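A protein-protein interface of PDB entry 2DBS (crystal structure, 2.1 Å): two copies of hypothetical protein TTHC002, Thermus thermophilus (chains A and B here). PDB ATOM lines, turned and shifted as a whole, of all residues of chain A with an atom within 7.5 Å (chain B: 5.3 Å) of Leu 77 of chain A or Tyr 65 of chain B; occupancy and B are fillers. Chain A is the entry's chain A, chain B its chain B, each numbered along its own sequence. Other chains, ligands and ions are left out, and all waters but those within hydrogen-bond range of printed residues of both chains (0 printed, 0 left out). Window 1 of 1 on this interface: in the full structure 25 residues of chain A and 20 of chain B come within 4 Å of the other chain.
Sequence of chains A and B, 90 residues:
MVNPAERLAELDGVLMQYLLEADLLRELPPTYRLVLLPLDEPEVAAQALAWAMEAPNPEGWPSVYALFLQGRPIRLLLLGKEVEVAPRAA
The side-chain hydroxyl (OH) of Tyr 65 of chain A lies within hydrogen-bond range of the guanidinium group (NH1) of Arg 75 of chain B, 3.4 Å away. N of Val 83 of chain B lies within hydrogen-bond range of O of Leu 76 of chain A (3.0 Å). The backbone NH (N) of Leu 78 of chain A lies within hydrogen-bond range of the backbone carbonyl oxygen (O) of Lys 81 of chain B (2.8 Å). The backbone carbonyl oxygen (O) of Val 83 of chain A is in hydrogen-bond range of the backbone NH (N) of Leu 76 of chain B, 2.7 Å away.
O of Ser 63 of chain A sits close to N of Leu 79 of chain A (3.4 Å). The backbone carbonyl oxygen (O) of Tyr 65 of chain A is in hydrogen-bond range of the backbone NH (N) of Leu 77 of chain A (2.9 Å). N of Leu 67 of chain A lies within hydrogen-bond range of O of Arg 75 of chain A (2.8 Å). The side-chain carboxylate (OE2) of Glu 82 of chain B lies within hydrogen-bond range of the side-chain hydroxyl (OG) of Ser 63 of chain B, at 3.3 Å. N of Leu 77 of chain B sits at hydrogen-bond distance from O of Tyr 65 of chain B, at 2.9 Å. The backbone NH of Leu 67 of chain B is in hydrogen-bond range of the backbone carbonyl oxygen of Arg 75 of chain B, 2.8 Å away.
Leu 77 of chain B touches Tyr 65 of chain A (CD2 to OH, 3.2 Å). CD1 of Leu 67 of chain A touches CD1 of Leu 49 of chain B, at 3.5 Å. NH1 of Arg 75 of chain A touches CD1 of Leu 49 of chain B, 3.0 Å away. CD of Arg 75 of chain A touches OH of Tyr 65 of chain B, 3.96 Å away. Glu 82 of chain B touches Arg 75 of chain A. Leu 77 of chain A touches Lys 81 of chain B. Leu 77 of chain B touches Leu 79 of chain A (CB to CD1, 3.9 Å). Lys 81 of chain A touches Leu 76 of chain B. Lys 81 of chain A touches Leu 77 of chain B. Arg 75 of chain B touches Val 83 of chain A.
Leu 77 of chain A touches just these residues of chain B: Tyr 65, Lys 81 and Glu 82. Of chain A, only Arg 75 (3.96 Å) and Leu 77 (3.4 Å) come within 4 Å of Tyr 65 of chain B. Of the printed residues of chain A, Leu 77 of chain B touches Tyr 65, Leu 79 and Lys 81. Printed residues of chain B within 4 Å of Lys 81 of chain A: Leu 76 and Leu 77. Of the printed residues of chain B, Leu 79 of chain A touches Leu 77. Of the printed residues of chain B, Leu 67 of chain A touches Leu 49 (3.5 Å). Printed residues of chain A within 4 Å of Leu 49 of chain B: Leu 67 (3.5 Å) and Arg 75 (3.0 Å). Val 35 of chain A touches none of the printed residues of chain B. The nearest residue of chain B that does not touch Leu 77 of chain A is Leu 77 of chain B (4.2 Å).
Printed residues of chain B that touch a printed residue of chain A: Leu 49, Tyr 65, Arg 75, Leu 76, Leu 77, Lys 81, Glu 82 and Val 83. Hydrophobic or aromatic side chains of chain B within 4 Å of the printed part of chain A: Leu 49, Tyr 65, Leu 76, Leu 77 and Val 83. Along chain B the printed residues that touch a printed residue of chain A span positions 49 to 83. Of the 17 printed residues of chain A, 9 touch a printed residue of chain B. Printed residues of chain A that touch a printed residue of chain B: Tyr 65, Leu 67, Arg 75, Leu 76, Leu 77, Leu 78, Leu 79, Lys 81 and Val 83. Among the printed residues, no Asp or Glu carboxylate lies within 4 Å of a Lys or Arg side-chain nitrogen of the other chain.
Tyr 65 of chain A touches Leu 77 of chain B, and with the chains exchanged Leu 77 of chain A touches Tyr 65 of chain B. Leu 76 of chain A touches Val 83 of chain B, and with the chains exchanged Val 83 of chain A touches Leu 76 of chain B. Leu 77 of chain A touches Lys 81 of chain B, and with the chains exchanged Lys 81 of chain A touches Leu 77 of chain B. Lys 81 of chain A touches Leu 76 of chain B, but with the chains exchanged Leu 76 of chain A does not touch Lys 81 of chain B (4.4 Å). Of the 18 pairs that touch across the chains among the printed residues, 10 have their exchanged pair printed and touching as well.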
ATOM      1  N   LEU A  28       0.328  13.222  -6.075  1.00  0.00           N
ATOM      2  CA  LEU A  28       0.851  13.352  -7.431  1.00  0.00           C
ATOM      3  C   LEU A  28       0.501  12.106  -8.225  1.00  0.00           C
ATOM      4  O   LEU A  28       0.420  11.016  -7.661  1.00  0.00           O
ATOM      5  CB  LEU A  28       2.374  13.516  -7.429  1.00  0.00           C
ATOM      6  CG  LEU A  28       2.994  14.781  -6.868  1.00  0.00           C
ATOM      7  CD1 LEU A  28       4.368  14.933  -7.461  1.00  0.00           C
ATOM      8  CD2 LEU A  28       2.138  15.982  -7.217  1.00  0.00           C
ATOM      9  N   VAL A  35       6.597  20.857 -13.810  1.00  0.00           N
ATOM     10  CA  VAL A  35       6.965  22.199 -14.234  1.00  0.00           C
ATOM     11  C   VAL A  35       7.276  22.903 -12.926  1.00  0.00           C
ATOM     12  O   VAL A  35       6.385  23.108 -12.107  1.00  0.00           O
ATOM     13  CB  VAL A  35       5.786  22.928 -14.946  1.00  0.00           C
ATOM     14  CG1 VAL A  35       6.199  24.326 -15.310  1.00  0.00           C
ATOM     15  CG2 VAL A  35       5.347  22.161 -16.182  1.00  0.00           C
ATOM     16  N   LEU A  37       8.108  26.185 -11.105  1.00  0.00           N
ATOM     17  CA  LEU A  37       8.054  27.630 -11.329  1.00  0.00           C
ATOM     18  C   LEU A  37       8.419  28.558 -10.149  1.00  0.00           C
ATOM     19  O   LEU A  37       7.595  28.828  -9.262  1.00  0.00           O
ATOM     20  CB  LEU A  37       6.662  28.014 -11.856  1.00  0.00           C
ATOM     21  CG  LEU A  37       6.225  27.514 -13.230  1.00  0.00           C
ATOM     22  CD1 LEU A  37       4.803  27.959 -13.523  1.00  0.00           C
ATOM     23  CD2 LEU A  37       7.184  28.055 -14.271  1.00  0.00           C
ATOM     24  N   LEU A  39       8.312  31.618  -8.700  1.00  0.00           N
ATOM     25  CA  LEU A  39       7.624  32.907  -8.869  1.00  0.00           C
ATOM     26  C   LEU A  39       8.463  34.142  -8.512  1.00  0.00           C
ATOM     27  O   LEU A  39       8.142  35.251  -8.928  1.00  0.00           O
ATOM     28  CB  LEU A  39       6.325  32.932  -8.055  1.00  0.00           C
ATOM     29  CG  LEU A  39       4.998  32.492  -8.688  1.00  0.00           C
ATOM     30  CD1 LEU A  39       5.189  32.028 -10.145  1.00  0.00           C
ATOM     31  CD2 LEU A  39       4.392  31.396  -7.833  1.00  0.00           C
ATOM     32  N   SER A  63       0.861  17.461 -16.500  1.00  0.00           N
ATOM     33  CA  SER A  63       1.750  18.435 -15.869  1.00  0.00           C
ATOM     34  C   SER A  63       1.415  18.670 -14.404  1.00  0.00           C
ATOM     35  O   SER A  63       0.249  18.636 -13.989  1.00  0.00           O
ATOM     36  CB  SER A  63       1.672  19.797 -16.570  1.00  0.00           C
ATOM     37  OG  SER A  63       2.332  19.815 -17.814  1.00  0.00           O
ATOM     38  N   VAL A  64       2.455  18.888 -13.619  1.00  0.00           N
ATOM     39  CA  VAL A  64       2.284  19.223 -12.217  1.00  0.00           C
ATOM     40  C   VAL A  64       3.139  20.464 -12.071  1.00  0.00           C
ATOM     41  O   VAL A  64       4.319  20.472 -12.437  1.00  0.00           O
ATOM     42  CB  VAL A  64       2.787  18.121 -11.241  1.00  0.00           C
ATOM     43  CG1 VAL A  64       2.933  18.709  -9.827  1.00  0.00           C
ATOM     44  CG2 VAL A  64       1.782  16.950 -11.203  1.00  0.00           C
ATOM     45  N   TYR A  65       2.542  21.533 -11.578  1.00  0.00           N
ATOM     46  CA  TYR A  65       3.291  22.749 -11.414  1.00  0.00           C
ATOM     47  C   TYR A  65       3.641  22.933  -9.960  1.00  0.00           C
ATOM     48  O   TYR A  65       2.786  22.829  -9.094  1.00  0.00           O
ATOM     49  CB  TYR A  65       2.474  23.930 -11.925  1.00  0.00           C
ATOM     50  CG  TYR A  65       2.243  23.872 -13.415  1.00  0.00           C
ATOM     51  CD1 TYR A  65       1.175  23.156 -13.945  1.00  0.00           C
ATOM     52  CD2 TYR A  65       3.115  24.522 -14.300  1.00  0.00           C
ATOM     53  CE1 TYR A  65       0.980  23.095 -15.314  1.00  0.00           C
ATOM     54  CE2 TYR A  65       2.923  24.460 -15.658  1.00  0.00           C
ATOM     55  CZ  TYR A  65       1.851  23.751 -16.158  1.00  0.00           C
ATOM     56  OH  TYR A  65       1.603  23.747 -17.494  1.00  0.00           O
ATOM     57  N   ALA A  66       4.914  23.197  -9.706  1.00  0.00           N
ATOM     58  CA  ALA A  66       5.415  23.411  -8.367  1.00  0.00           C
ATOM     59  C   ALA A  66       5.746  24.896  -8.219  1.00  0.00           C
ATOM     60  O   ALA A  66       6.786  25.360  -8.671  1.00  0.00           O
ATOM     61  CB  ALA A  66       6.659  22.564  -8.155  1.00  0.00           C
ATOM     62  N   LEU A  67       4.855  25.647  -7.593  1.00  0.00           N
ATOM     63  CA  LEU A  67       5.089  27.069  -7.411  1.00  0.00           C
ATOM     64  C   LEU A  67       6.054  27.260  -6.272  1.00  0.00           C
ATOM     65  O   LEU A  67       5.776  26.860  -5.148  1.00  0.00           O
ATOM     66  CB  LEU A  67       3.778  27.781  -7.099  1.00  0.00           C
ATOM     67  CG  LEU A  67       2.556  27.294  -7.872  1.00  0.00           C
ATOM     68  CD1 LEU A  67       1.409  28.216  -7.521  1.00  0.00           C
ATOM     69  CD2 LEU A  67       2.809  27.267  -9.386  1.00  0.00           C
ATOM     70  N   ARG A  75       3.187  25.716  -3.334  1.00  0.00           N
ATOM     71  CA  ARG A  75       1.948  25.098  -3.770  1.00  0.00           C
ATOM     72  C   ARG A  75       2.111  24.264  -5.026  1.00  0.00           C
ATOM     73  O   ARG A  75       2.934  24.578  -5.875  1.00  0.00           O
ATOM     74  CB  ARG A  75       0.882  26.160  -4.012  1.00  0.00           C
ATOM     75  CG  ARG A  75      -0.270  25.676  -4.879  1.00  0.00           C
ATOM     76  CD  ARG A  75      -1.453  26.547  -4.670  1.00  0.00           C
ATOM     77  NE  ARG A  75      -1.625  26.747  -3.240  1.00  0.00           N
ATOM     78  CZ  ARG A  75      -1.471  27.917  -2.627  1.00  0.00           C
ATOM     79  NH1 ARG A  75      -1.150  29.002  -3.331  1.00  0.00           N
ATOM     80  NH2 ARG A  75      -1.608  27.989  -1.308  1.00  0.00           N
ATOM     81  N   LEU A  76       1.305  23.212  -5.137  1.00  0.00           N
ATOM     82  CA  LEU A  76       1.312  22.308  -6.291  1.00  0.00           C
ATOM     83  C   LEU A  76      -0.037  22.411  -6.997  1.00  0.00           C
ATOM     84  O   LEU A  76      -1.065  22.369  -6.337  1.00  0.00           O
ATOM     85  CB  LEU A  76       1.496  20.858  -5.833  1.00  0.00           C
ATOM     86  CG  LEU A  76       2.753  20.053  -6.176  1.00  0.00           C
ATOM     87  CD1 LEU A  76       4.020  20.864  -5.935  1.00  0.00           C
ATOM     88  CD2 LEU A  76       2.752  18.802  -5.319  1.00  0.00           C
ATOM     89  N   LEU A  77      -0.035  22.560  -8.323  1.00  0.00           N
ATOM     90  CA  LEU A  77      -1.272  22.622  -9.094  1.00  0.00           C
ATOM     91  C   LEU A  77      -1.348  21.322  -9.887  1.00  0.00           C
ATOM     92  O   LEU A  77      -0.470  21.026 -10.688  1.00  0.00           O
ATOM     93  CB  LEU A  77      -1.276  23.811 -10.065  1.00  0.00           C
ATOM     94  CG  LEU A  77      -0.732  25.161  -9.612  1.00  0.00           C
ATOM     95  CD1 LEU A  77      -1.228  26.203 -10.552  1.00  0.00           C
ATOM     96  CD2 LEU A  77      -1.179  25.500  -8.202  1.00  0.00           C
ATOM     97  N   LEU A  78      -2.384  20.530  -9.640  1.00  0.00           N
ATOM     98  CA  LEU A  78      -2.543  19.269 -10.354  1.00  0.00           C
ATOM     99  C   LEU A  78      -3.429  19.556 -11.546  1.00  0.00           C
ATOM    100  O   LEU A  78      -4.618  19.848 -11.413  1.00  0.00           O
ATOM    101  CB  LEU A  78      -3.176  18.199  -9.469  1.00  0.00           C
ATOM    102  CG  LEU A  78      -2.562  16.806  -9.673  1.00  0.00           C
ATOM    103  CD1 LEU A  78      -2.822  16.282 -11.102  1.00  0.00           C
ATOM    104  CD2 LEU A  78      -1.066  16.890  -9.396  1.00  0.00           C
ATOM    105  N   LEU A  79      -2.833  19.458 -12.720  1.00  0.00           N
ATOM    106  CA  LEU A  79      -3.535  19.788 -13.929  1.00  0.00           C
ATOM    107  C   LEU A  79      -4.780  19.022 -14.316  1.00  0.00           C
ATOM    108  O   LEU A  79      -4.894  17.803 -14.135  1.00  0.00           O
ATOM    109  CB  LEU A  79      -2.559  19.774 -15.098  1.00  0.00           C
ATOM    110  CG  LEU A  79      -2.356  21.118 -15.783  1.00  0.00           C
ATOM    111  CD1 LEU A  79      -2.005  22.194 -14.771  1.00  0.00           C
ATOM    112  CD2 LEU A  79      -1.267  20.949 -16.800  1.00  0.00           C
ATOM    113  N   GLY A  80      -5.718  19.808 -14.839  1.00  0.00           N
ATOM    114  CA  GLY A  80      -6.970  19.320 -15.363  1.00  0.00           C
ATOM    115  C   GLY A  80      -6.723  19.548 -16.848  1.00  0.00           C
ATOM    116  O   GLY A  80      -6.647  18.613 -17.640  1.00  0.00           O
ATOM    117  N   LYS A  81      -6.552  20.806 -17.224  1.00  0.00           N
ATOM    118  CA  LYS A  81      -6.278  21.124 -18.607  1.00  0.00           C
ATOM    119  C   LYS A  81      -5.385  22.331 -18.743  1.00  0.00           C
ATOM    120  O   LYS A  81      -5.240  23.115 -17.823  1.00  0.00           O
ATOM    121  CB  LYS A  81      -7.576  21.349 -19.374  1.00  0.00           C
ATOM    122  CG  LYS A  81      -7.913  20.200 -20.325  1.00  0.00           C
ATOM    123  CD  LYS A  81      -7.193  20.316 -21.691  1.00  0.00           C
ATOM    124  CE  LYS A  81      -5.661  20.519 -21.606  1.00  0.00           C
ATOM    125  NZ  LYS A  81      -4.901  19.429 -20.926  1.00  0.00           N
ATOM    126  N   VAL A  83      -4.133  25.511 -21.608  1.00  0.00           N
ATOM    127  CA  VAL A  83      -4.616  26.277 -22.737  1.00  0.00           C
ATOM    128  C   VAL A  83      -3.541  27.246 -23.159  1.00  0.00           C
ATOM    129  O   VAL A  83      -3.097  28.068 -22.369  1.00  0.00           O
ATOM    130  CB  VAL A  83      -5.862  27.072 -22.360  1.00  0.00           C
ATOM    131  CG1 VAL A  83      -6.341  27.871 -23.550  1.00  0.00           C
ATOM    132  CG2 VAL A  83      -6.945  26.130 -21.871  1.00  0.00           C
ATOM    133  N   VAL B  35      -6.503  33.329 -10.987  1.00  0.00           N
ATOM    134  CA  VAL B  35      -5.250  33.628 -10.328  1.00  0.00           C
ATOM    135  C   VAL B  35      -4.271  34.027 -11.426  1.00  0.00           C
ATOM    136  O   VAL B  35      -3.849  33.189 -12.223  1.00  0.00           O
ATOM    137  CB  VAL B  35      -4.703  32.401  -9.567  1.00  0.00           C
ATOM    138  CG1 VAL B  35      -3.574  32.824  -8.671  1.00  0.00           C
ATOM    139  CG2 VAL B  35      -5.820  31.745  -8.758  1.00  0.00           C
ATOM    140  N   LEU B  37      -0.736  35.019 -12.607  1.00  0.00           N
ATOM    141  CA  LEU B  37       0.652  34.941 -12.160  1.00  0.00           C
ATOM    142  C   LEU B  37       1.696  35.446 -13.148  1.00  0.00           C
ATOM    143  O   LEU B  37       2.125  34.722 -14.047  1.00  0.00           O
ATOM    144  CB  LEU B  37       1.022  33.512 -11.760  1.00  0.00           C
ATOM    145  CG  LEU B  37       0.263  32.902 -10.597  1.00  0.00           C
ATOM    146  CD1 LEU B  37       0.862  31.553 -10.297  1.00  0.00           C
ATOM    147  CD2 LEU B  37       0.324  33.797  -9.387  1.00  0.00           C
ATOM    148  N   LEU B  49      -0.473  35.085  -5.493  1.00  0.00           N
ATOM    149  CA  LEU B  49      -0.567  33.754  -4.874  1.00  0.00           C
ATOM    150  C   LEU B  49      -0.992  33.896  -3.412  1.00  0.00           C
ATOM    151  O   LEU B  49      -1.679  33.036  -2.875  1.00  0.00           O
ATOM    152  CB  LEU B  49       0.764  32.970  -4.963  1.00  0.00           C
ATOM    153  CG  LEU B  49       0.696  31.468  -4.572  1.00  0.00           C
ATOM    154  CD1 LEU B  49      -0.168  30.706  -5.569  1.00  0.00           C
ATOM    155  CD2 LEU B  49       2.092  30.841  -4.517  1.00  0.00           C
ATOM    156  N   ALA B  52      -4.588  33.993  -3.274  1.00  0.00           N
ATOM    157  CA  ALA B  52      -5.166  32.709  -3.654  1.00  0.00           C
ATOM    158  C   ALA B  52      -5.042  31.742  -2.477  1.00  0.00           C
ATOM    159  O   ALA B  52      -5.825  30.798  -2.349  1.00  0.00           O
ATOM    160  CB  ALA B  52      -4.451  32.150  -4.869  1.00  0.00           C
ATOM    161  N   SER B  63     -10.196  27.148  -9.512  1.00  0.00           N
ATOM    162  CA  SER B  63      -9.134  28.074  -9.896  1.00  0.00           C
ATOM    163  C   SER B  63      -8.734  28.004 -11.370  1.00  0.00           C
ATOM    164  O   SER B  63      -8.752  26.941 -12.012  1.00  0.00           O
ATOM    165  CB  SER B  63      -7.883  27.843  -9.033  1.00  0.00           C
ATOM    166  OG  SER B  63      -8.176  27.915  -7.647  1.00  0.00           O
ATOM    167  N   VAL B  64      -8.385  29.171 -11.891  1.00  0.00           N
ATOM    168  CA  VAL B  64      -7.930  29.311 -13.256  1.00  0.00           C
ATOM    169  C   VAL B  64      -6.641  30.111 -13.151  1.00  0.00           C
ATOM    170  O   VAL B  64      -6.648  31.237 -12.675  1.00  0.00           O
ATOM    171  CB  VAL B  64      -8.957  30.071 -14.131  1.00  0.00           C
ATOM    172  CG1 VAL B  64      -8.345  30.390 -15.511  1.00  0.00           C
ATOM    173  CG2 VAL B  64     -10.240  29.230 -14.277  1.00  0.00           C
ATOM    174  N   TYR B  65      -5.533  29.502 -13.562  1.00  0.00           N
ATOM    175  CA  TYR B  65      -4.244  30.159 -13.520  1.00  0.00           C
ATOM    176  C   TYR B  65      -3.913  30.725 -14.879  1.00  0.00           C
ATOM    177  O   TYR B  65      -3.960  30.010 -15.858  1.00  0.00           O
ATOM    178  CB  TYR B  65      -3.153  29.161 -13.117  1.00  0.00           C
ATOM    179  CG  TYR B  65      -2.994  29.026 -11.628  1.00  0.00           C
ATOM    180  CD1 TYR B  65      -3.900  28.282 -10.877  1.00  0.00           C
ATOM    181  CD2 TYR B  65      -1.994  29.736 -10.954  1.00  0.00           C
ATOM    182  CE1 TYR B  65      -3.823  28.258  -9.485  1.00  0.00           C
ATOM    183  CE2 TYR B  65      -1.909  29.721  -9.580  1.00  0.00           C
ATOM    184  CZ  TYR B  65      -2.825  28.988  -8.850  1.00  0.00           C
ATOM    185  OH  TYR B  65      -2.765  29.005  -7.484  1.00  0.00           O
ATOM    186  N   ALA B  66      -3.569  32.006 -14.930  1.00  0.00           N
ATOM    187  CA  ALA B  66      -3.208  32.658 -16.166  1.00  0.00           C
ATOM    188  C   ALA B  66      -1.751  33.040 -16.035  1.00  0.00           C
ATOM    189  O   ALA B  66      -1.421  33.988 -15.329  1.00  0.00           O
ATOM    190  CB  ALA B  66      -4.056  33.886 -16.360  1.00  0.00           C
ATOM    191  N   LEU B  67      -0.876  32.287 -16.697  1.00  0.00           N
ATOM    192  CA  LEU B  67       0.569  32.551 -16.648  1.00  0.00           C
ATOM    193  C   LEU B  67       0.935  33.651 -17.632  1.00  0.00           C
ATOM    194  O   LEU B  67       0.736  33.511 -18.832  1.00  0.00           O
ATOM    195  CB  LEU B  67       1.368  31.286 -16.957  1.00  0.00           C
ATOM    196  CG  LEU B  67       1.194  30.112 -15.986  1.00  0.00           C
ATOM    197  CD1 LEU B  67       1.942  28.883 -16.496  1.00  0.00           C
ATOM    198  CD2 LEU B  67       1.699  30.505 -14.610  1.00  0.00           C
ATOM    199  N   ARG B  75      -0.276  31.236 -21.122  1.00  0.00           N
ATOM    200  CA  ARG B  75      -0.953  29.961 -20.959  1.00  0.00           C
ATOM    201  C   ARG B  75      -1.944  29.971 -19.801  1.00  0.00           C
ATOM    202  O   ARG B  75      -1.765  30.703 -18.835  1.00  0.00           O
ATOM    203  CB  ARG B  75       0.077  28.843 -20.762  1.00  0.00           C
ATOM    204  CG  ARG B  75      -0.534  27.510 -20.384  1.00  0.00           C
ATOM    205  CD  ARG B  75       0.527  26.454 -20.209  1.00  0.00           C
ATOM    206  NE  ARG B  75       0.990  25.923 -21.481  1.00  0.00           N
ATOM    207  CZ  ARG B  75       2.046  25.125 -21.616  1.00  0.00           C
ATOM    208  NH1 ARG B  75       2.749  24.769 -20.554  1.00  0.00           N
ATOM    209  NH2 ARG B  75       2.401  24.686 -22.821  1.00  0.00           N
ATOM    210  N   LEU B  76      -2.993  29.158 -19.918  1.00  0.00           N
ATOM    211  CA  LEU B  76      -4.017  29.038 -18.888  1.00  0.00           C
ATOM    212  C   LEU B  76      -4.065  27.584 -18.376  1.00  0.00           C
ATOM    213  O   LEU B  76      -4.132  26.652 -19.172  1.00  0.00           O
ATOM    214  CB  LEU B  76      -5.393  29.425 -19.449  1.00  0.00           C
ATOM    215  CG  LEU B  76      -5.720  30.799 -20.060  1.00  0.00           C
ATOM    216  CD1 LEU B  76      -7.212  30.882 -20.208  1.00  0.00           C
ATOM    217  CD2 LEU B  76      -5.279  31.949 -19.183  1.00  0.00           C
ATOM    218  N   LEU B  77      -4.022  27.394 -17.056  1.00  0.00           N
ATOM    219  CA  LEU B  77      -4.060  26.061 -16.449  1.00  0.00           C
ATOM    220  C   LEU B  77      -5.430  25.893 -15.817  1.00  0.00           C
ATOM    221  O   LEU B  77      -5.785  26.634 -14.902  1.00  0.00           O
ATOM    222  CB  LEU B  77      -2.977  25.945 -15.375  1.00  0.00           C
ATOM    223  CG  LEU B  77      -1.637  26.531 -15.835  1.00  0.00           C
ATOM    224  CD1 LEU B  77      -0.765  26.885 -14.673  1.00  0.00           C
ATOM    225  CD2 LEU B  77      -0.945  25.537 -16.761  1.00  0.00           C
ATOM    226  N   LYS B  81      -6.987  19.780  -9.420  1.00  0.00           N
ATOM    227  CA  LYS B  81      -6.870  19.828  -7.972  1.00  0.00           C
ATOM    228  C   LYS B  81      -5.701  20.695  -7.545  1.00  0.00           C
ATOM    229  O   LYS B  81      -4.772  20.937  -8.305  1.00  0.00           O
ATOM    230  CB  LYS B  81      -6.706  18.423  -7.383  1.00  0.00           C
ATOM    231  CG  LYS B  81      -8.017  17.642  -7.193  1.00  0.00           C
ATOM    232  CD  LYS B  81      -7.766  16.376  -6.376  1.00  0.00           C
ATOM    233  CE  LYS B  81      -8.962  15.440  -6.375  1.00  0.00           C
ATOM    234  NZ  LYS B  81      -8.612  14.094  -5.812  1.00  0.00           N
ATOM    235  N   GLU B  82      -5.769  21.166  -6.311  1.00  0.00           N
ATOM    236  CA  GLU B  82      -4.735  22.010  -5.746  1.00  0.00           C
ATOM    237  C   GLU B  82      -4.197  21.256  -4.538  1.00  0.00           C
ATOM    238  O   GLU B  82      -4.903  20.444  -3.944  1.00  0.00           O
ATOM    239  CB  GLU B  82      -5.334  23.336  -5.303  1.00  0.00           C
ATOM    240  CG  GLU B  82      -4.434  24.538  -5.438  1.00  0.00           C
ATOM    241  CD  GLU B  82      -4.655  25.277  -6.746  1.00  0.00           C
ATOM    242  OE1 GLU B  82      -3.984  24.938  -7.743  1.00  0.00           O
ATOM    243  OE2 GLU B  82      -5.508  26.193  -6.788  1.00  0.00           O
ATOM    244  N   VAL B  83      -2.948  21.524  -4.179  1.00  0.00           N
ATOM    245  CA  VAL B  83      -2.318  20.855  -3.054  1.00  0.00           C
ATOM    246  C   VAL B  83      -1.419  21.827  -2.308  1.00  0.00           C
ATOM    247  O   VAL B  83      -0.485  22.369  -2.881  1.00  0.00           O
ATOM    248  CB  VAL B  83      -1.466  19.671  -3.529  1.00  0.00           C
ATOM    249  CG1 VAL B  83      -0.974  18.877  -2.339  1.00  0.00           C
ATOM    250  CG2 VAL B  83      -2.270  18.791  -4.482  1.00  0.00           C
